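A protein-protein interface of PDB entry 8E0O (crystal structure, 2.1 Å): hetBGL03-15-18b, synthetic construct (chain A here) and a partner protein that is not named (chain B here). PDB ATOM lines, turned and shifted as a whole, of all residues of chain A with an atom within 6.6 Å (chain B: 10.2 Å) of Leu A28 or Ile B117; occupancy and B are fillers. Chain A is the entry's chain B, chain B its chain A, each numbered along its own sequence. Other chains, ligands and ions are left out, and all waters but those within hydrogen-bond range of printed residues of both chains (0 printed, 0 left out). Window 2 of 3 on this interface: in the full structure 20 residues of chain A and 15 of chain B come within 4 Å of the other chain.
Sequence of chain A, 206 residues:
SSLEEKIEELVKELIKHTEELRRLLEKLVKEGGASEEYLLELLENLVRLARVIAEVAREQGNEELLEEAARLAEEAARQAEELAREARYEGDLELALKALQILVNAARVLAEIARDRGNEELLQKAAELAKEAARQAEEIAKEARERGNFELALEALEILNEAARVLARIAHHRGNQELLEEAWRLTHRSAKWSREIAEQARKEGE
No residue of chain B comes within 4 Å of Leu A25.
No residue of chain B comes within 4 Å of Glu A26.
Leu A28 touches one residue of chain B.
No residue of chain B comes within 4 Å of Val A29.
No residue of chain B comes within 4 Å of Glu A31.
No residue of chain B comes within 4 Å of Gly A32.
Of the printed residues of chain B, Tyr A38 touches Ile B117, Glu B118 and Leu B121.
Of the printed residues of chain B, Glu A41 touches Leu B121 (3.6 Å) and Lys B122 (3.1 Å).
Ile B117 touches three residues of chain A.
The nearest residue of chain A that does not touch Ile B117 is Leu A21 (4.5 Å).
Of the 13 printed residues of chain A, 5 touch a printed residue of chain B.
Hydrophobic or aromatic side chains of chain A that line the printed part of chain B: Leu A21, Leu A24, Leu A28 and Tyr A38.
NH2 of Arg B61 is in salt-bridge range of OE1 of Glu B118 (2.6 Å).
The side-chain amide nitrogen (NE2) of Gln B112 lies within hydrogen-bond range of the side-chain hydroxyl (OG) of Ser B108 (3.1 Å).
The side-chain carboxylate (OE2) of Glu B118 lies within salt-bridge range of the side-chain amino group (NZ) of Lys B122 (3.1 Å).
Among the printed residues, merely in contact across the chains: Glu A41 with Lys B122 (3.1 Å), Tyr A38 with Glu B118 (3.4 Å), Leu A28 with Ile B117 (3.5 Å), Glu A41 with Leu B121 (3.6 Å), Tyr A38 with Leu B121 (3.6 Å), Leu A21 with Asn B124 (3.7 Å), Leu A24 with Ile B117 (3.7 Å), Leu A24 with Gln B112 (3.7 Å), Tyr A38 with Ile B117 (3.9 Å) and Leu A21 with Leu B121 (3.96 Å).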
ATOM      1  N   LEU A  21      31.111 -19.102  15.149  1.00  0.00           N
ATOM      2  CA  LEU A  21      31.011 -19.922  13.946  1.00  0.00           C
ATOM      3  C   LEU A  21      31.736 -19.266  12.778  1.00  0.00           C
ATOM      4  O   LEU A  21      32.361 -19.951  11.960  1.00  0.00           O
ATOM      5  CB  LEU A  21      29.544 -20.170  13.597  1.00  0.00           C
ATOM      6  CG  LEU A  21      29.291 -21.099  12.408  1.00  0.00           C
ATOM      7  CD1 LEU A  21      29.971 -22.444  12.622  1.00  0.00           C
ATOM      8  CD2 LEU A  21      27.799 -21.279  12.168  1.00  0.00           C
ATOM      9  N   ARG A  23      34.373 -17.352  13.118  1.00  0.00           N
ATOM     10  CA  ARG A  23      35.787 -17.572  13.405  1.00  0.00           C
ATOM     11  C   ARG A  23      36.201 -18.995  13.059  1.00  0.00           C
ATOM     12  O   ARG A  23      37.325 -19.232  12.600  1.00  0.00           O
ATOM     13  CB  ARG A  23      36.074 -17.273  14.877  1.00  0.00           C
ATOM     14  CG  ARG A  23      36.843 -15.983  15.118  1.00  0.00           C
ATOM     15  CD  ARG A  23      36.028 -14.765  14.715  1.00  0.00           C
ATOM     16  N   LEU A  24      35.302 -19.959  13.271  1.00  0.00           N
ATOM     17  CA  LEU A  24      35.616 -21.348  12.953  1.00  0.00           C
ATOM     18  C   LEU A  24      35.745 -21.552  11.450  1.00  0.00           C
ATOM     19  O   LEU A  24      36.663 -22.239  10.987  1.00  0.00           O
ATOM     20  CB  LEU A  24      34.547 -22.273  13.536  1.00  0.00           C
ATOM     21  CG  LEU A  24      34.670 -23.761  13.202  1.00  0.00           C
ATOM     22  CD1 LEU A  24      35.784 -24.405  14.010  1.00  0.00           C
ATOM     23  CD2 LEU A  24      33.350 -24.474  13.450  1.00  0.00           C
ATOM     24  N   LEU A  25      34.839 -20.957  10.672  1.00  0.00           N
ATOM     25  CA  LEU A  25      34.934 -21.061   9.221  1.00  0.00           C
ATOM     26  C   LEU A  25      36.128 -20.286   8.682  1.00  0.00           C
ATOM     27  O   LEU A  25      36.727 -20.695   7.681  1.00  0.00           O
ATOM     28  CB  LEU A  25      33.641 -20.564   8.573  1.00  0.00           C
ATOM     29  N   GLU A  26      36.488 -19.174   9.326  1.00  0.00           N
ATOM     30  CA  GLU A  26      37.653 -18.414   8.889  1.00  0.00           C
ATOM     31  C   GLU A  26      38.930 -19.224   9.072  1.00  0.00           C
ATOM     32  O   GLU A  26      39.802 -19.232   8.197  1.00  0.00           O
ATOM     33  CB  GLU A  26      37.736 -17.090   9.652  1.00  0.00           C
ATOM     34  N   LYS A  27      39.055 -19.918  10.204  1.00  0.00           N
ATOM     35  CA  LYS A  27      40.210 -20.777  10.434  1.00  0.00           C
ATOM     36  C   LYS A  27      40.177 -22.045   9.591  1.00  0.00           C
ATOM     37  O   LYS A  27      41.182 -22.764   9.550  1.00  0.00           O
ATOM     38  CB  LYS A  27      40.305 -21.142  11.918  1.00  0.00           C
ATOM     39  N   LEU A  28      39.062 -22.336   8.921  1.00  0.00           N
ATOM     40  CA  LEU A  28      38.971 -23.500   8.050  1.00  0.00           C
ATOM     41  C   LEU A  28      39.391 -23.205   6.616  1.00  0.00           C
ATOM     42  O   LEU A  28      39.488 -24.139   5.814  1.00  0.00           O
ATOM     43  CB  LEU A  28      37.549 -24.070   8.067  1.00  0.00           C
ATOM     44  CG  LEU A  28      37.397 -25.380   8.846  1.00  0.00           C
ATOM     45  CD1 LEU A  28      38.069 -25.303  10.210  1.00  0.00           C
ATOM     46  CD2 LEU A  28      35.938 -25.759   8.988  1.00  0.00           C
ATOM     47  N   VAL A  29      39.632 -21.937   6.275  1.00  0.00           N
ATOM     48  CA  VAL A  29      40.255 -21.616   4.998  1.00  0.00           C
ATOM     49  C   VAL A  29      41.724 -22.015   4.997  1.00  0.00           C
ATOM     50  O   VAL A  29      42.344 -22.102   3.931  1.00  0.00           O
ATOM     51  CB  VAL A  29      40.102 -20.117   4.679  1.00  0.00           C
ATOM     52  N   LYS A  30      42.298 -22.258   6.178  1.00  0.00           N
ATOM     53  CA  LYS A  30      43.696 -22.665   6.272  1.00  0.00           C
ATOM     54  C   LYS A  30      43.943 -23.999   5.578  1.00  0.00           C
ATOM     55  O   LYS A  30      45.073 -24.282   5.164  1.00  0.00           O
ATOM     56  CB  LYS A  30      44.108 -22.730   7.744  1.00  0.00           C
ATOM     57  CG  LYS A  30      44.033 -24.114   8.355  1.00  0.00           C
ATOM     58  CD  LYS A  30      44.218 -24.047   9.857  1.00  0.00           C
ATOM     59  CE  LYS A  30      43.693 -25.306  10.521  1.00  0.00           C
ATOM     60  NZ  LYS A  30      43.915 -25.300  11.992  1.00  0.00           N
ATOM     61  N   GLU A  31      42.907 -24.827   5.436  1.00  0.00           N
ATOM     62  CA  GLU A  31      43.028 -26.114   4.768  1.00  0.00           C
ATOM     63  C   GLU A  31      41.924 -26.369   3.751  1.00  0.00           C
ATOM     64  O   GLU A  31      41.905 -27.444   3.142  1.00  0.00           O
ATOM     65  CB  GLU A  31      43.039 -27.255   5.798  1.00  0.00           C
ATOM     66  N   GLY A  32      41.009 -25.426   3.552  1.00  0.00           N
ATOM     67  CA  GLY A  32      39.926 -25.600   2.604  1.00  0.00           C
ATOM     68  C   GLY A  32      38.743 -26.354   3.177  1.00  0.00           C
ATOM     69  O   GLY A  32      38.499 -27.507   2.822  1.00  0.00           O
ATOM     70  N   TYR A  38      29.341 -23.921   2.018  1.00  0.00           N
ATOM     71  CA  TYR A  38      29.150 -23.614   3.429  1.00  0.00           C
ATOM     72  C   TYR A  38      29.447 -22.157   3.758  1.00  0.00           C
ATOM     73  O   TYR A  38      29.003 -21.671   4.803  1.00  0.00           O
ATOM     74  CB  TYR A  38      30.013 -24.543   4.286  1.00  0.00           C
ATOM     75  CG  TYR A  38      29.629 -25.998   4.143  1.00  0.00           C
ATOM     76  CD1 TYR A  38      30.593 -26.996   4.123  1.00  0.00           C
ATOM     77  CD2 TYR A  38      28.295 -26.372   4.022  1.00  0.00           C
ATOM     78  CE1 TYR A  38      30.240 -28.328   3.989  1.00  0.00           C
ATOM     79  CE2 TYR A  38      27.933 -27.699   3.888  1.00  0.00           C
ATOM     80  CZ  TYR A  38      28.909 -28.673   3.872  1.00  0.00           C
ATOM     81  OH  TYR A  38      28.553 -29.995   3.739  1.00  0.00           O
ATOM     82  N   GLU A  41      26.072 -20.531   2.917  1.00  0.00           N
ATOM     83  CA  GLU A  41      25.098 -20.840   3.957  1.00  0.00           C
ATOM     84  C   GLU A  41      25.335 -20.000   5.205  1.00  0.00           C
ATOM     85  O   GLU A  41      24.379 -19.590   5.873  1.00  0.00           O
ATOM     86  CB  GLU A  41      25.142 -22.327   4.298  1.00  0.00           C
ATOM     87  CG  GLU A  41      24.016 -22.760   5.211  1.00  0.00           C
ATOM     88  CD  GLU A  41      23.917 -24.261   5.346  1.00  0.00           C
ATOM     89  OE1 GLU A  41      24.698 -24.977   4.684  1.00  0.00           O
ATOM     90  OE2 GLU A  41      23.052 -24.722   6.117  1.00  0.00           O
ATOM     91  N   ARG B  61      21.681 -34.659  13.766  1.00  0.00           N
ATOM     92  CA  ARG B  61      20.833 -34.120  12.708  1.00  0.00           C
ATOM     93  C   ARG B  61      19.361 -34.365  13.011  1.00  0.00           C
ATOM     94  O   ARG B  61      18.528 -33.465  12.849  1.00  0.00           O
ATOM     95  CB  ARG B  61      21.212 -34.729  11.358  1.00  0.00           C
ATOM     96  CG  ARG B  61      20.286 -34.323  10.221  1.00  0.00           C
ATOM     97  CD  ARG B  61      20.675 -34.996   8.914  1.00  0.00           C
ATOM     98  NE  ARG B  61      22.109 -34.917   8.663  1.00  0.00           N
ATOM     99  CZ  ARG B  61      22.694 -33.957   7.960  1.00  0.00           C
ATOM    100  NH1 ARG B  61      21.995 -32.971   7.420  1.00  0.00           N
ATOM    101  NH2 ARG B  61      24.013 -33.986   7.793  1.00  0.00           N
ATOM    102  N   LEU B  64      18.275 -32.023  15.854  1.00  0.00           N
ATOM    103  CA  LEU B  64      17.998 -30.653  15.431  1.00  0.00           C
ATOM    104  C   LEU B  64      16.641 -30.548  14.746  1.00  0.00           C
ATOM    105  O   LEU B  64      15.939 -29.542  14.899  1.00  0.00           O
ATOM    106  CB  LEU B  64      19.107 -30.156  14.504  1.00  0.00           C
ATOM    107  CG  LEU B  64      20.428 -29.776  15.174  1.00  0.00           C
ATOM    108  CD1 LEU B  64      21.513 -29.555  14.130  1.00  0.00           C
ATOM    109  CD2 LEU B  64      20.255 -28.542  16.047  1.00  0.00           C
ATOM    110  N   ILE B 107      24.093 -28.619  21.273  1.00  0.00           N
ATOM    111  CA  ILE B 107      24.405 -29.389  20.073  1.00  0.00           C
ATOM    112  C   ILE B 107      25.317 -28.590  19.148  1.00  0.00           C
ATOM    113  O   ILE B 107      26.255 -29.138  18.557  1.00  0.00           O
ATOM    114  CB  ILE B 107      23.106 -29.818  19.367  1.00  0.00           C
ATOM    115  CG1 ILE B 107      22.384 -30.891  20.185  1.00  0.00           C
ATOM    116  CG2 ILE B 107      23.390 -30.327  17.962  1.00  0.00           C
ATOM    117  CD1 ILE B 107      20.946 -31.110  19.769  1.00  0.00           C
ATOM    118  N   SER B 108      25.070 -27.284  19.022  1.00  0.00           N
ATOM    119  CA  SER B 108      25.886 -26.453  18.143  1.00  0.00           C
ATOM    120  C   SER B 108      27.338 -26.412  18.604  1.00  0.00           C
ATOM    121  O   SER B 108      28.260 -26.407  17.779  1.00  0.00           O
ATOM    122  CB  SER B 108      25.310 -25.041  18.070  1.00  0.00           C
ATOM    123  OG  SER B 108      26.096 -24.221  17.227  1.00  0.00           O
ATOM    124  N   LYS B 109      27.565 -26.378  19.920  1.00  0.00           N
ATOM    125  CA  LYS B 109      28.932 -26.381  20.429  1.00  0.00           C
ATOM    126  C   LYS B 109      29.603 -27.729  20.197  1.00  0.00           C
ATOM    127  O   LYS B 109      30.798 -27.788  19.887  1.00  0.00           O
ATOM    128  CB  LYS B 109      28.940 -26.023  21.915  1.00  0.00           C
ATOM    129  N   ARG B 110      28.850 -28.822  20.340  1.00  0.00           N
ATOM    130  CA  ARG B 110      29.414 -30.146  20.099  1.00  0.00           C
ATOM    131  C   ARG B 110      29.743 -30.343  18.624  1.00  0.00           C
ATOM    132  O   ARG B 110      30.749 -30.980  18.285  1.00  0.00           O
ATOM    133  CB  ARG B 110      28.447 -31.224  20.587  1.00  0.00           C
ATOM    134  CG  ARG B 110      28.887 -32.646  20.281  1.00  0.00           C
ATOM    135  CD  ARG B 110      29.952 -33.118  21.257  1.00  0.00           C
ATOM    136  NE  ARG B 110      29.378 -33.839  22.387  1.00  0.00           N
ATOM    137  CZ  ARG B 110      29.908 -34.926  22.931  1.00  0.00           C
ATOM    138  NH1 ARG B 110      31.031 -35.452  22.470  1.00  0.00           N
ATOM    139  NH2 ARG B 110      29.295 -35.501  23.962  1.00  0.00           N
ATOM    140  N   LEU B 111      28.912 -29.801  17.731  1.00  0.00           N
ATOM    141  CA  LEU B 111      29.186 -29.917  16.303  1.00  0.00           C
ATOM    142  C   LEU B 111      30.407 -29.095  15.907  1.00  0.00           C
ATOM    143  O   LEU B 111      31.205 -29.526  15.066  1.00  0.00           O
ATOM    144  CB  LEU B 111      27.962 -29.485  15.496  1.00  0.00           C
ATOM    145  CG  LEU B 111      26.728 -30.381  15.615  1.00  0.00           C
ATOM    146  CD1 LEU B 111      25.503 -29.679  15.054  1.00  0.00           C
ATOM    147  CD2 LEU B 111      26.961 -31.710  14.913  1.00  0.00           C
ATOM    148  N   GLN B 112      30.568 -27.910  16.500  1.00  0.00           N
ATOM    149  CA  GLN B 112      31.724 -27.078  16.185  1.00  0.00           C
ATOM    150  C   GLN B 112      33.016 -27.715  16.685  1.00  0.00           C
ATOM    151  O   GLN B 112      34.063 -27.595  16.041  1.00  0.00           O
ATOM    152  CB  GLN B 112      31.542 -25.682  16.783  1.00  0.00           C
ATOM    153  CG  GLN B 112      30.628 -24.778  15.970  1.00  0.00           C
ATOM    154  CD  GLN B 112      30.183 -23.549  16.741  1.00  0.00           C
ATOM    155  OE1 GLN B 112      30.953 -22.968  17.505  1.00  0.00           O
ATOM    156  NE2 GLN B 112      28.933 -23.147  16.542  1.00  0.00           N
ATOM    157  N   GLU B 113      32.958 -28.399  17.831  1.00  0.00           N
ATOM    158  CA  GLU B 113      34.140 -29.091  18.337  1.00  0.00           C
ATOM    159  C   GLU B 113      34.518 -30.261  17.438  1.00  0.00           C
ATOM    160  O   GLU B 113      35.707 -30.518  17.212  1.00  0.00           O
ATOM    161  CB  GLU B 113      33.895 -29.572  19.767  1.00  0.00           C
ATOM    162  CG  GLU B 113      34.083 -28.500  20.825  1.00  0.00           C
ATOM    163  CD  GLU B 113      33.569 -28.931  22.184  1.00  0.00           C
ATOM    164  OE1 GLU B 113      32.919 -29.994  22.266  1.00  0.00           O
ATOM    165  OE2 GLU B 113      33.818 -28.208  23.171  1.00  0.00           O
ATOM    166  N   GLU B 114      33.523 -30.978  16.917  1.00  0.00           N
ATOM    167  CA  GLU B 114      33.767 -32.102  16.023  1.00  0.00           C
ATOM    168  C   GLU B 114      34.152 -31.672  14.614  1.00  0.00           C
ATOM    169  O   GLU B 114      34.494 -32.531  13.795  1.00  0.00           O
ATOM    170  CB  GLU B 114      32.528 -32.999  15.953  1.00  0.00           C
ATOM    171  CG  GLU B 114      32.264 -33.809  17.211  1.00  0.00           C
ATOM    172  CD  GLU B 114      30.852 -34.361  17.257  1.00  0.00           C
ATOM    173  OE1 GLU B 114      30.142 -34.268  16.235  1.00  0.00           O
ATOM    174  OE2 GLU B 114      30.451 -34.889  18.316  1.00  0.00           O
ATOM    175  N   GLY B 115      34.102 -30.377  14.311  1.00  0.00           N
ATOM    176  CA  GLY B 115      34.375 -29.924  12.963  1.00  0.00           C
ATOM    177  C   GLY B 115      33.272 -30.212  11.972  1.00  0.00           C
ATOM    178  O   GLY B 115      33.502 -30.137  10.762  1.00  0.00           O
ATOM    179  N   ASN B 116      32.075 -30.543  12.451  1.00  0.00           N
ATOM    180  CA  ASN B 116      30.935 -30.844  11.587  1.00  0.00           C
ATOM    181  C   ASN B 116      30.292 -29.523  11.183  1.00  0.00           C
ATOM    182  O   ASN B 116      29.386 -29.017  11.845  1.00  0.00           O
ATOM    183  CB  ASN B 116      29.951 -31.760  12.304  1.00  0.00           C
ATOM    184  CG  ASN B 116      28.977 -32.433  11.357  1.00  0.00           C
ATOM    185  OD1 ASN B 116      28.636 -31.890  10.306  1.00  0.00           O
ATOM    186  ND2 ASN B 116      28.522 -33.625  11.728  1.00  0.00           N
ATOM    187  N   ILE B 117      30.764 -28.961  10.069  1.00  0.00           N
ATOM    188  CA  ILE B 117      30.346 -27.619   9.673  1.00  0.00           C
ATOM    189  C   ILE B 117      28.943 -27.627   9.081  1.00  0.00           C
ATOM    190  O   ILE B 117      28.147 -26.715   9.340  1.00  0.00           O
ATOM    191  CB  ILE B 117      31.374 -27.014   8.701  1.00  0.00           C
ATOM    192  CG1 ILE B 117      32.580 -26.498   9.485  1.00  0.00           C
ATOM    193  CG2 ILE B 117      30.751 -25.906   7.857  1.00  0.00           C
ATOM    194  CD1 ILE B 117      32.452 -25.056   9.926  1.00  0.00           C
ATOM    195  N   GLU B 118      28.615 -28.644   8.280  1.00  0.00           N
ATOM    196  CA  GLU B 118      27.280 -28.718   7.695  1.00  0.00           C
ATOM    197  C   GLU B 118      26.209 -28.701   8.778  1.00  0.00           C
ATOM    198  O   GLU B 118      25.265 -27.906   8.722  1.00  0.00           O
ATOM    199  CB  GLU B 118      27.148 -29.970   6.831  1.00  0.00           C
ATOM    200  CG  GLU B 118      25.878 -30.000   5.997  1.00  0.00           C
ATOM    201  CD  GLU B 118      25.142 -31.322   6.104  1.00  0.00           C
ATOM    202  OE1 GLU B 118      25.640 -32.225   6.809  1.00  0.00           O
ATOM    203  OE2 GLU B 118      24.064 -31.456   5.485  1.00  0.00           O
ATOM    204  N   LEU B 119      26.353 -29.564   9.785  1.00  0.00           N
ATOM    205  CA  LEU B 119      25.373 -29.607  10.864  1.00  0.00           C
ATOM    206  C   LEU B 119      25.476 -28.387  11.770  1.00  0.00           C
ATOM    207  O   LEU B 119      24.463 -27.944  12.324  1.00  0.00           O
ATOM    208  CB  LEU B 119      25.541 -30.893  11.674  1.00  0.00           C
ATOM    209  CG  LEU B 119      24.730 -32.112  11.225  1.00  0.00           C
ATOM    210  CD1 LEU B 119      24.518 -33.070  12.388  1.00  0.00           C
ATOM    211  CD2 LEU B 119      23.395 -31.694  10.627  1.00  0.00           C
ATOM    212  N   ALA B 120      26.680 -27.832  11.936  1.00  0.00           N
ATOM    213  CA  ALA B 120      26.823 -26.620  12.737  1.00  0.00           C
ATOM    214  C   ALA B 120      26.101 -25.441  12.101  1.00  0.00           C
ATOM    215  O   ALA B 120      25.566 -24.586  12.817  1.00  0.00           O
ATOM    216  CB  ALA B 120      28.300 -26.285  12.945  1.00  0.00           C
ATOM    217  N   LEU B 121      26.074 -25.376  10.768  1.00  0.00           N
ATOM    218  CA  LEU B 121      25.330 -24.317  10.095  1.00  0.00           C
ATOM    219  C   LEU B 121      23.831 -24.487  10.297  1.00  0.00           C
ATOM    220  O   LEU B 121      23.119 -23.504  10.536  1.00  0.00           O
ATOM    221  CB  LEU B 121      25.676 -24.297   8.606  1.00  0.00           C
ATOM    222  CG  LEU B 121      27.086 -23.821   8.249  1.00  0.00           C
ATOM    223  CD1 LEU B 121      27.449 -24.263   6.842  1.00  0.00           C
ATOM    224  CD2 LEU B 121      27.201 -22.312   8.392  1.00  0.00           C
ATOM    225  N   LYS B 122      23.333 -25.723  10.203  1.00  0.00           N
ATOM    226  CA  LYS B 122      21.921 -25.977  10.481  1.00  0.00           C
ATOM    227  C   LYS B 122      21.574 -25.614  11.920  1.00  0.00           C
ATOM    228  O   LYS B 122      20.515 -25.031  12.184  1.00  0.00           O
ATOM    229  CB  LYS B 122      21.576 -27.445  10.214  1.00  0.00           C
ATOM    230  CG  LYS B 122      22.143 -28.046   8.932  1.00  0.00           C
ATOM    231  CD  LYS B 122      21.828 -27.214   7.702  1.00  0.00           C
ATOM    232  CE  LYS B 122      22.556 -27.754   6.478  1.00  0.00           C
ATOM    233  NZ  LYS B 122      22.119 -29.130   6.125  1.00  0.00           N
ATOM    234  N   ALA B 123      22.453 -25.956  12.864  1.00  0.00           N
ATOM    235  CA  ALA B 123      22.192 -25.651  14.266  1.00  0.00           C
ATOM    236  C   ALA B 123      22.175 -24.148  14.513  1.00  0.00           C
ATOM    237  O   ALA B 123      21.341 -23.650  15.280  1.00  0.00           O
ATOM    238  CB  ALA B 123      23.234 -26.330  15.156  1.00  0.00           C
ATOM    239  N   ASN B 124      23.085 -23.409  13.873  1.00  0.00           N
ATOM    240  CA  ASN B 124      23.103 -21.959  14.034  1.00  0.00           C
ATOM    241  C   ASN B 124      21.854 -21.323  13.438  1.00  0.00           C
ATOM    242  O   ASN B 124      21.307 -20.368  14.002  1.00  0.00           O
ATOM    243  CB  ASN B 124      24.362 -21.376  13.395  1.00  0.00           C
ATOM    244  CG  ASN B 124      24.414 -19.862  13.481  1.00  0.00           C
ATOM    245  OD1 ASN B 124      24.283 -19.167  12.472  1.00  0.00           O
ATOM    246  ND2 ASN B 124      24.608 -19.343  14.688  1.00  0.00           N
ATOM    247  N   ARG B 125      21.388 -21.837  12.296  1.00  0.00           N
ATOM    248  CA  ARG B 125      20.152 -21.334  11.709  1.00  0.00           C
ATOM    249  C   ARG B 125      18.969 -21.556  12.644  1.00  0.00           C
ATOM    250  O   ARG B 125      18.141 -20.657  12.836  1.00  0.00           O
ATOM    251  CB  ARG B 125      19.901 -22.004  10.358  1.00  0.00           C
ATOM    252  CG  ARG B 125      18.575 -21.635   9.706  1.00  0.00           C
ATOM    253  CD  ARG B 125      18.483 -20.142   9.421  1.00  0.00           C
ATOM    254  NE  ARG B 125      17.310 -19.811   8.622  1.00  0.00           N
ATOM    255  CZ  ARG B 125      16.751 -18.609   8.575  1.00  0.00           C
